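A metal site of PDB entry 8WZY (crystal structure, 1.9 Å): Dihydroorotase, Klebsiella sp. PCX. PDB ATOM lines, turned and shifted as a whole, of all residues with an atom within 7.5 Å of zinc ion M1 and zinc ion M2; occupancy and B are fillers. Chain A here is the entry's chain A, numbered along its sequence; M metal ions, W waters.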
ATOM      1  N   HIS A  56     -16.013  22.407 -12.749  1.00  0.00           N
ATOM      2  CA  HIS A  56     -15.406  21.333 -13.522  1.00  0.00           C
ATOM      3  C   HIS A  56     -15.810  19.999 -12.890  1.00  0.00           C
ATOM      4  O   HIS A  56     -15.093  19.485 -12.030  1.00  0.00           O
ATOM      5  CB  HIS A  56     -13.899  21.474 -13.593  1.00  0.00           C
ATOM      6  CG  HIS A  56     -13.237  20.510 -14.517  1.00  0.00           C
ATOM      7  ND1 HIS A  56     -12.033  20.765 -15.129  1.00  0.00           N
ATOM      8  CD2 HIS A  56     -13.622  19.277 -14.943  1.00  0.00           C
ATOM      9  CE1 HIS A  56     -11.706  19.743 -15.899  1.00  0.00           C
ATOM     10  NE2 HIS A  56     -12.650  18.823 -15.799  1.00  0.00           N
ATOM     11  N   VAL A  57     -16.950  19.468 -13.306  1.00  0.00           N
ATOM     12  CA  VAL A  57     -17.411  18.160 -12.853  1.00  0.00           C
ATOM     13  C   VAL A  57     -17.757  17.322 -14.078  1.00  0.00           C
ATOM     14  O   VAL A  57     -17.819  17.817 -15.198  1.00  0.00           O
ATOM     15  CB  VAL A  57     -18.631  18.240 -11.921  1.00  0.00           C
ATOM     16  CG1 VAL A  57     -18.363  19.155 -10.729  1.00  0.00           C
ATOM     17  CG2 VAL A  57     -19.891  18.654 -12.702  1.00  0.00           C
ATOM     18  N   HIS A  58     -18.005  16.039 -13.830  1.00  0.00           N
ATOM     19  CA  HIS A  58     -18.606  15.145 -14.825  1.00  0.00           C
ATOM     20  C   HIS A  58     -19.808  14.469 -14.195  1.00  0.00           C
ATOM     21  O   HIS A  58     -19.663  13.492 -13.452  1.00  0.00           O
ATOM     22  CB  HIS A  58     -17.600  14.133 -15.340  1.00  0.00           C
ATOM     23  CG  HIS A  58     -16.478  14.766 -16.068  1.00  0.00           C
ATOM     24  ND1 HIS A  58     -16.641  15.343 -17.305  1.00  0.00           N
ATOM     25  CD2 HIS A  58     -15.197  14.996 -15.704  1.00  0.00           C
ATOM     26  CE1 HIS A  58     -15.490  15.872 -17.695  1.00  0.00           C
ATOM     27  NE2 HIS A  58     -14.604  15.667 -16.742  1.00  0.00           N
ATOM     28  N   TYR A  66     -16.608   8.621 -17.288  1.00  0.00           N
ATOM     29  CA  TYR A  66     -16.649   9.711 -16.318  1.00  0.00           C
ATOM     30  C   TYR A  66     -18.107  10.120 -16.137  1.00  0.00           C
ATOM     31  O   TYR A  66     -18.595  11.065 -16.755  1.00  0.00           O
ATOM     32  CB  TYR A  66     -15.752  10.857 -16.752  1.00  0.00           C
ATOM     33  CG  TYR A  66     -14.402  10.367 -17.210  1.00  0.00           C
ATOM     34  CD1 TYR A  66     -13.438  10.002 -16.287  1.00  0.00           C
ATOM     35  CD2 TYR A  66     -14.088  10.276 -18.569  1.00  0.00           C
ATOM     36  CE1 TYR A  66     -12.200   9.529 -16.698  1.00  0.00           C
ATOM     37  CE2 TYR A  66     -12.856   9.819 -18.978  1.00  0.00           C
ATOM     38  CZ  TYR A  66     -11.911   9.445 -18.043  1.00  0.00           C
ATOM     39  OH  TYR A  66     -10.678   8.984 -18.428  1.00  0.00           O
ATOM     40  N   ASP A  84     -20.730  20.871 -15.818  1.00  0.00           N
ATOM     41  CA  ASP A  84     -20.188  19.694 -16.460  1.00  0.00           C
ATOM     42  C   ASP A  84     -19.205  20.100 -17.547  1.00  0.00           C
ATOM     43  O   ASP A  84     -19.541  20.879 -18.441  1.00  0.00           O
ATOM     44  CB  ASP A  84     -21.317  18.833 -17.039  1.00  0.00           C
ATOM     45  CG  ASP A  84     -20.801  17.583 -17.752  1.00  0.00           C
ATOM     46  OD1 ASP A  84     -20.543  16.564 -17.080  1.00  0.00           O
ATOM     47  OD2 ASP A  84     -20.650  17.633 -18.991  1.00  0.00           O
ATOM     48  N   ALA A  85     -18.001  19.545 -17.470  1.00  0.00           N
ATOM     49  CA  ALA A  85     -16.872  20.032 -18.277  1.00  0.00           C
ATOM     50  C   ALA A  85     -16.760  19.212 -19.561  1.00  0.00           C
ATOM     51  O   ALA A  85     -15.792  18.492 -19.815  1.00  0.00           O
ATOM     52  CB  ALA A  85     -15.589  19.985 -17.461  1.00  0.00           C
ATOM     53  N   GLY A  86     -17.790  19.350 -20.396  1.00  0.00           N
ATOM     54  CA  GLY A  86     -17.758  18.720 -21.692  1.00  0.00           C
ATOM     55  C   GLY A  86     -17.879  17.213 -21.711  1.00  0.00           C
ATOM     56  O   GLY A  86     -17.254  16.570 -22.554  1.00  0.00           O
ATOM     57  N   SER A  87     -18.679  16.631 -20.794  1.00  0.00           N
ATOM     58  CA  SER A  87     -18.982  15.202 -20.883  1.00  0.00           C
ATOM     59  C   SER A  87     -19.790  14.888 -22.136  1.00  0.00           C
ATOM     60  O   SER A  87     -19.648  13.804 -22.716  1.00  0.00           O
ATOM     61  CB  SER A  87     -19.751  14.748 -19.640  1.00  0.00           C
ATOM     62  OG  SER A  87     -19.045  15.037 -18.451  1.00  0.00           O
ATOM     63  N   LEU A 118     -17.505  12.762 -24.232  1.00  0.00           N
ATOM     64  CA  LEU A 118     -16.635  11.791 -23.595  1.00  0.00           C
ATOM     65  C   LEU A 118     -17.136  10.358 -23.783  1.00  0.00           C
ATOM     66  O   LEU A 118     -16.793   9.476 -22.970  1.00  0.00           O
ATOM     67  CB  LEU A 118     -16.455  12.114 -22.114  1.00  0.00           C
ATOM     68  CG  LEU A 118     -15.771  13.469 -21.856  1.00  0.00           C
ATOM     69  CD1 LEU A 118     -15.538  13.723 -20.370  1.00  0.00           C
ATOM     70  CD2 LEU A 118     -14.477  13.580 -22.652  1.00  0.00           C
ATOM     71  N   KCX A 150     -15.794  23.202 -24.198  1.00  0.00           N
ATOM     72  CA  KCX A 150     -14.714  22.449 -23.576  1.00  0.00           C
ATOM     73  CB  KCX A 150     -15.263  21.327 -22.682  1.00  0.00           C
ATOM     74  CG  KCX A 150     -14.468  21.021 -21.395  1.00  0.00           C
ATOM     75  CD  KCX A 150     -13.024  20.679 -21.637  1.00  0.00           C
ATOM     76  CE  KCX A 150     -12.296  20.390 -20.328  1.00  0.00           C
ATOM     77  NZ  KCX A 150     -12.857  19.126 -19.739  1.00  0.00           N
ATOM     78  C   KCX A 150     -13.812  21.863 -24.655  1.00  0.00           C
ATOM     79  O   KCX A 150     -14.304  21.240 -25.601  1.00  0.00           O
ATOM     80  CX  KCX A 150     -12.134  18.236 -19.070  1.00  0.00           C
ATOM     81  OQ1 KCX A 150     -12.709  17.220 -18.639  1.00  0.00           O
ATOM     82  OQ2 KCX A 150     -10.915  18.372 -18.870  1.00  0.00           O
ATOM     83  N   ALA A 151     -12.511  22.050 -24.528  1.00  0.00           N
ATOM     84  CA  ALA A 151     -11.577  21.405 -25.434  1.00  0.00           C
ATOM     85  C   ALA A 151     -10.464  20.740 -24.632  1.00  0.00           C
ATOM     86  O   ALA A 151      -9.761  21.418 -23.890  1.00  0.00           O
ATOM     87  CB  ALA A 151     -10.998  22.400 -26.438  1.00  0.00           C
ATOM     88  N   ARG A 152     -10.325  19.418 -24.751  1.00  0.00           N
ATOM     89  CA  ARG A 152      -9.285  18.690 -24.026  1.00  0.00           C
ATOM     90  C   ARG A 152      -8.063  18.557 -24.925  1.00  0.00           C
ATOM     91  O   ARG A 152      -7.974  17.648 -25.759  1.00  0.00           O
ATOM     92  CB  ARG A 152      -9.789  17.312 -23.570  1.00  0.00           C
ATOM     93  CG  ARG A 152     -11.073  17.367 -22.739  1.00  0.00           C
ATOM     94  CD  ARG A 152     -11.253  16.089 -21.927  1.00  0.00           C
ATOM     95  NE  ARG A 152     -11.336  14.917 -22.798  1.00  0.00           N
ATOM     96  CZ  ARG A 152     -10.792  13.742 -22.528  1.00  0.00           C
ATOM     97  NH1 ARG A 152     -10.103  13.538 -21.421  1.00  0.00           N
ATOM     98  NH2 ARG A 152     -10.955  12.740 -23.402  1.00  0.00           N
ATOM     99  N   MET A 153      -7.104  19.460 -24.756  1.00  0.00           N
ATOM    100  CA  MET A 153      -5.993  19.571 -25.691  1.00  0.00           C
ATOM    101  C   MET A 153      -4.798  18.831 -25.104  1.00  0.00           C
ATOM    102  O   MET A 153      -3.943  19.419 -24.445  1.00  0.00           O
ATOM    103  CB  MET A 153      -5.685  21.031 -25.989  1.00  0.00           C
ATOM    104  CG  MET A 153      -6.909  21.740 -26.526  1.00  0.00           C
ATOM    105  SD  MET A 153      -7.199  21.316 -28.233  1.00  0.00           S
ATOM    106  CE  MET A 153      -5.537  21.261 -28.898  1.00  0.00           C
ATOM    107  N   SER A 154      -4.745  17.529 -25.346  1.00  0.00           N
ATOM    108  CA  SER A 154      -3.644  16.702 -24.880  1.00  0.00           C
ATOM    109  C   SER A 154      -3.429  15.564 -25.874  1.00  0.00           C
ATOM    110  O   SER A 154      -4.227  15.375 -26.795  1.00  0.00           O
ATOM    111  CB  SER A 154      -3.874  16.171 -23.460  1.00  0.00           C
ATOM    112  OG  SER A 154      -5.121  15.505 -23.360  1.00  0.00           O
ATOM    113  N   VAL A 157      -6.026  12.762 -26.823  1.00  0.00           N
ATOM    114  CA  VAL A 157      -7.325  13.267 -27.235  1.00  0.00           C
ATOM    115  C   VAL A 157      -7.302  13.772 -28.673  1.00  0.00           C
ATOM    116  O   VAL A 157      -8.219  13.508 -29.449  1.00  0.00           O
ATOM    117  CB  VAL A 157      -7.818  14.369 -26.275  1.00  0.00           C
ATOM    118  CG1 VAL A 157      -9.252  14.761 -26.612  1.00  0.00           C
ATOM    119  CG2 VAL A 157      -7.715  13.889 -24.837  1.00  0.00           C
ATOM    120  N   MET A 182     -13.161  26.476 -21.977  1.00  0.00           N
ATOM    121  CA  MET A 182     -12.292  25.775 -21.041  1.00  0.00           C
ATOM    122  C   MET A 182     -11.393  24.804 -21.791  1.00  0.00           C
ATOM    123  O   MET A 182     -11.866  23.984 -22.577  1.00  0.00           O
ATOM    124  CB  MET A 182     -13.112  25.023 -19.984  1.00  0.00           C
ATOM    125  CG  MET A 182     -12.248  24.270 -19.010  1.00  0.00           C
ATOM    126  SD  MET A 182     -13.180  23.435 -17.705  1.00  0.00           S
ATOM    127  CE  MET A 182     -13.361  24.796 -16.560  1.00  0.00           C
ATOM    128  N   VAL A 183     -10.085  24.921 -21.551  1.00  0.00           N
ATOM    129  CA  VAL A 183      -9.070  24.155 -22.246  1.00  0.00           C
ATOM    130  C   VAL A 183      -8.372  23.293 -21.213  1.00  0.00           C
ATOM    131  O   VAL A 183      -7.821  23.807 -20.230  1.00  0.00           O
ATOM    132  CB  VAL A 183      -8.062  25.079 -22.954  1.00  0.00           C
ATOM    133  CG1 VAL A 183      -7.038  24.247 -23.725  1.00  0.00           C
ATOM    134  CG2 VAL A 183      -8.798  26.047 -23.880  1.00  0.00           C
ATOM    135  N   HIS A 184      -8.428  21.978 -21.408  1.00  0.00           N
ATOM    136  CA  HIS A 184      -7.700  21.040 -20.577  1.00  0.00           C
ATOM    137  C   HIS A 184      -6.281  20.898 -21.098  1.00  0.00           C
ATOM    138  O   HIS A 184      -6.044  20.912 -22.312  1.00  0.00           O
ATOM    139  CB  HIS A 184      -8.474  19.711 -20.523  1.00  0.00           C
ATOM    140  CG  HIS A 184      -7.660  18.474 -20.731  1.00  0.00           C
ATOM    141  ND1 HIS A 184      -7.837  17.344 -19.952  1.00  0.00           N
ATOM    142  CD2 HIS A 184      -6.751  18.122 -21.669  1.00  0.00           C
ATOM    143  CE1 HIS A 184      -7.032  16.389 -20.371  1.00  0.00           C
ATOM    144  NE2 HIS A 184      -6.354  16.830 -21.408  1.00  0.00           N
ATOM    145  N   ILE A 185      -5.323  20.790 -20.175  1.00  0.00           N
ATOM    146  CA  ILE A 185      -3.911  20.593 -20.510  1.00  0.00           C
ATOM    147  C   ILE A 185      -3.382  19.406 -19.709  1.00  0.00           C
ATOM    148  O   ILE A 185      -3.927  19.034 -18.662  1.00  0.00           O
ATOM    149  CB  ILE A 185      -3.062  21.856 -20.246  1.00  0.00           C
ATOM    150  CG1 ILE A 185      -3.155  22.258 -18.766  1.00  0.00           C
ATOM    151  CG2 ILE A 185      -3.482  22.993 -21.164  1.00  0.00           C
ATOM    152  CD1 ILE A 185      -2.041  23.192 -18.296  1.00  0.00           C
ATOM    153  N   THR A 206      -7.820  24.706 -17.473  1.00  0.00           N
ATOM    154  CA  THR A 206      -8.046  23.830 -16.326  1.00  0.00           C
ATOM    155  C   THR A 206      -6.916  22.807 -16.211  1.00  0.00           C
ATOM    156  O   THR A 206      -6.052  22.695 -17.084  1.00  0.00           O
ATOM    157  CB  THR A 206      -9.427  23.173 -16.427  1.00  0.00           C
ATOM    158  OG1 THR A 206      -9.766  22.557 -15.178  1.00  0.00           O
ATOM    159  CG2 THR A 206      -9.472  22.127 -17.554  1.00  0.00           C
ATOM    160  N   HIS A 207      -6.917  22.062 -15.092  1.00  0.00           N
ATOM    161  CA  HIS A 207      -5.768  21.249 -14.655  1.00  0.00           C
ATOM    162  C   HIS A 207      -4.521  22.097 -14.494  1.00  0.00           C
ATOM    163  O   HIS A 207      -3.415  21.678 -14.832  1.00  0.00           O
ATOM    164  CB  HIS A 207      -5.502  20.065 -15.595  1.00  0.00           C
ATOM    165  CG  HIS A 207      -6.716  19.285 -15.925  1.00  0.00           C
ATOM    166  ND1 HIS A 207      -7.679  18.983 -14.985  1.00  0.00           N
ATOM    167  CD2 HIS A 207      -7.150  18.746 -17.088  1.00  0.00           C
ATOM    168  CE1 HIS A 207      -8.647  18.287 -15.557  1.00  0.00           C
ATOM    169  NE2 HIS A 207      -8.341  18.124 -16.827  1.00  0.00           N
ATOM    170  N   GLY A 240      -9.251  22.066 -11.496  1.00  0.00           N
ATOM    171  CA  GLY A 240      -9.670  20.788 -12.063  1.00  0.00           C
ATOM    172  C   GLY A 240      -8.861  19.609 -11.570  1.00  0.00           C
ATOM    173  O   GLY A 240      -8.284  18.864 -12.382  1.00  0.00           O
ATOM    174  N   GLY A 242      -9.022  16.388 -10.357  1.00  0.00           N
ATOM    175  CA  GLY A 242      -9.084  15.146 -11.090  1.00  0.00           C
ATOM    176  C   GLY A 242      -8.253  14.029 -10.506  1.00  0.00           C
ATOM    177  O   GLY A 242      -7.698  14.107  -9.408  1.00  0.00           O
ATOM    178  N   SER A 245      -4.459  15.185 -12.438  1.00  0.00           N
ATOM    179  CA  SER A 245      -4.237  16.557 -12.886  1.00  0.00           C
ATOM    180  C   SER A 245      -3.846  17.535 -11.783  1.00  0.00           C
ATOM    181  O   SER A 245      -3.834  18.743 -12.031  1.00  0.00           O
ATOM    182  CB  SER A 245      -5.481  17.096 -13.600  1.00  0.00           C
ATOM    183  OG  SER A 245      -5.716  16.391 -14.804  1.00  0.00           O
ATOM    184  N   SER A 266     -12.918  20.503  -9.032  1.00  0.00           N
ATOM    185  CA  SER A 266     -12.579  19.171  -8.555  1.00  0.00           C
ATOM    186  C   SER A 266     -12.244  18.192  -9.674  1.00  0.00           C
ATOM    187  O   SER A 266     -11.454  17.261  -9.434  1.00  0.00           O
ATOM    188  CB  SER A 266     -13.745  18.597  -7.747  1.00  0.00           C
ATOM    189  OG  SER A 266     -14.898  18.522  -8.560  1.00  0.00           O
ATOM    190  N   ASP A 267     -12.810  18.371 -10.867  1.00  0.00           N
ATOM    191  CA  ASP A 267     -12.764  17.360 -11.933  1.00  0.00           C
ATOM    192  C   ASP A 267     -13.259  16.015 -11.394  1.00  0.00           C
ATOM    193  O   ASP A 267     -12.665  14.963 -11.607  1.00  0.00           O
ATOM    194  CB  ASP A 267     -11.373  17.239 -12.538  1.00  0.00           C
ATOM    195  CG  ASP A 267     -11.353  16.357 -13.783  1.00  0.00           C
ATOM    196  OD1 ASP A 267     -12.427  16.127 -14.372  1.00  0.00           O
ATOM    197  OD2 ASP A 267     -10.264  15.860 -14.132  1.00  0.00           O
ATOM    198  N   ILE A 268     -14.401  16.080 -10.718  1.00  0.00           N
ATOM    199  CA  ILE A 268     -14.923  14.953  -9.962  1.00  0.00           C
ATOM    200  C   ILE A 268     -15.832  14.104 -10.855  1.00  0.00           C
ATOM    201  O   ILE A 268     -16.564  14.616 -11.698  1.00  0.00           O
ATOM    202  CB  ILE A 268     -15.659  15.458  -8.714  1.00  0.00           C
ATOM    203  CG1 ILE A 268     -15.974  14.324  -7.733  1.00  0.00           C
ATOM    204  CG2 ILE A 268     -16.934  16.219  -9.093  1.00  0.00           C
ATOM    205  CD1 ILE A 268     -16.423  14.835  -6.356  1.00  0.00           C
ATOM    206  N   TYR A 269     -15.748  12.791 -10.674  1.00  0.00           N
ATOM    207  CA  TYR A 269     -16.746  11.871 -11.179  1.00  0.00           C
ATOM    208  C   TYR A 269     -16.857  10.752 -10.160  1.00  0.00           C
ATOM    209  O   TYR A 269     -16.187  10.781  -9.127  1.00  0.00           O
ATOM    210  CB  TYR A 269     -16.424  11.410 -12.599  1.00  0.00           C
ATOM    211  CG  TYR A 269     -15.327  10.389 -12.693  1.00  0.00           C
ATOM    212  CD1 TYR A 269     -13.998  10.752 -12.525  1.00  0.00           C
ATOM    213  CD2 TYR A 269     -15.603   9.068 -13.023  1.00  0.00           C
ATOM    214  CE1 TYR A 269     -12.989   9.837 -12.622  1.00  0.00           C
ATOM    215  CE2 TYR A 269     -14.595   8.136 -13.135  1.00  0.00           C
ATOM    216  CZ  TYR A 269     -13.288   8.517 -12.931  1.00  0.00           C
ATOM    217  OH  TYR A 269     -12.275   7.592 -13.038  1.00  0.00           O
HETATM  218 ZN    ZN M   1      -9.496  17.051 -18.417  1.00  0.00          ZN
HETATM  219 ZN    ZN M   2     -12.636  16.725 -16.612  1.00  0.00          ZN
HETATM  220  O   HOH W   1     -10.410  14.408 -18.478  1.00  0.00           O
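A ring nitrogen (NE2) of His 184 is in hydrogen-bond range of the side-chain hydroxyl (OG) of Ser 154 (2.7 Å). The side-chain hydroxyl (OG1) of Thr 206 lies within hydrogen-bond range of a ring nitrogen (ND1) of His 56 (2.9 Å). A ring nitrogen (ND1) of His 207 sits close to the side-chain hydroxyl (OG) of Ser 245. The backbone carbonyl oxygen of Ile 268 is in hydrogen-bond range of the backbone NH of His 58 (2.9 Å). The backbone carbonyl oxygen (O) of Ala 85 is in hydrogen-bond range of NZ of KCX 150. A ring nitrogen (ND1) of His 58 lies within hydrogen-bond range of the side-chain hydroxyl of Ser 87 (2.7 Å). The backbone carbonyl oxygen (O) of Ala 151 is in hydrogen-bond range of the backbone NH (N) of His 184 (2.9 Å). The backbone NH (N) of Met 153 lies within hydrogen-bond range of the backbone carbonyl oxygen (O) of His 184.
Of the 28 residues printed, 3 come within 4 Å of zinc ion M1. The nearest printed residue that does not touch zinc ion M1 is Arg 152 (4.04 Å).
Of the 28 residues printed, 4 come within 4 Å of zinc ion M2.
Zinc ion M1 is bound by OQ2 of KCX 150 (2.0 Å), NE2 of His 207 (2.2 Å) and ND1 of His 184 (2.3 Å). Zinc ion M1 has three donor atoms within binding distance. Slightly farther from zinc ion M1 lies water W1 (2.8 Å).
OQ1 of KCX 150 is bound to zinc ion M2 (2.1 Å). NE2 of His 58 is bound to zinc ion M2 (2.2 Å). A ring nitrogen (NE2) of His 56 binds zinc ion M2, at 2.3 Å. OD1 of Asp 267 binds zinc ion M2, at 2.3 Å. Zinc ion M2 has four donor atoms within binding distance.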
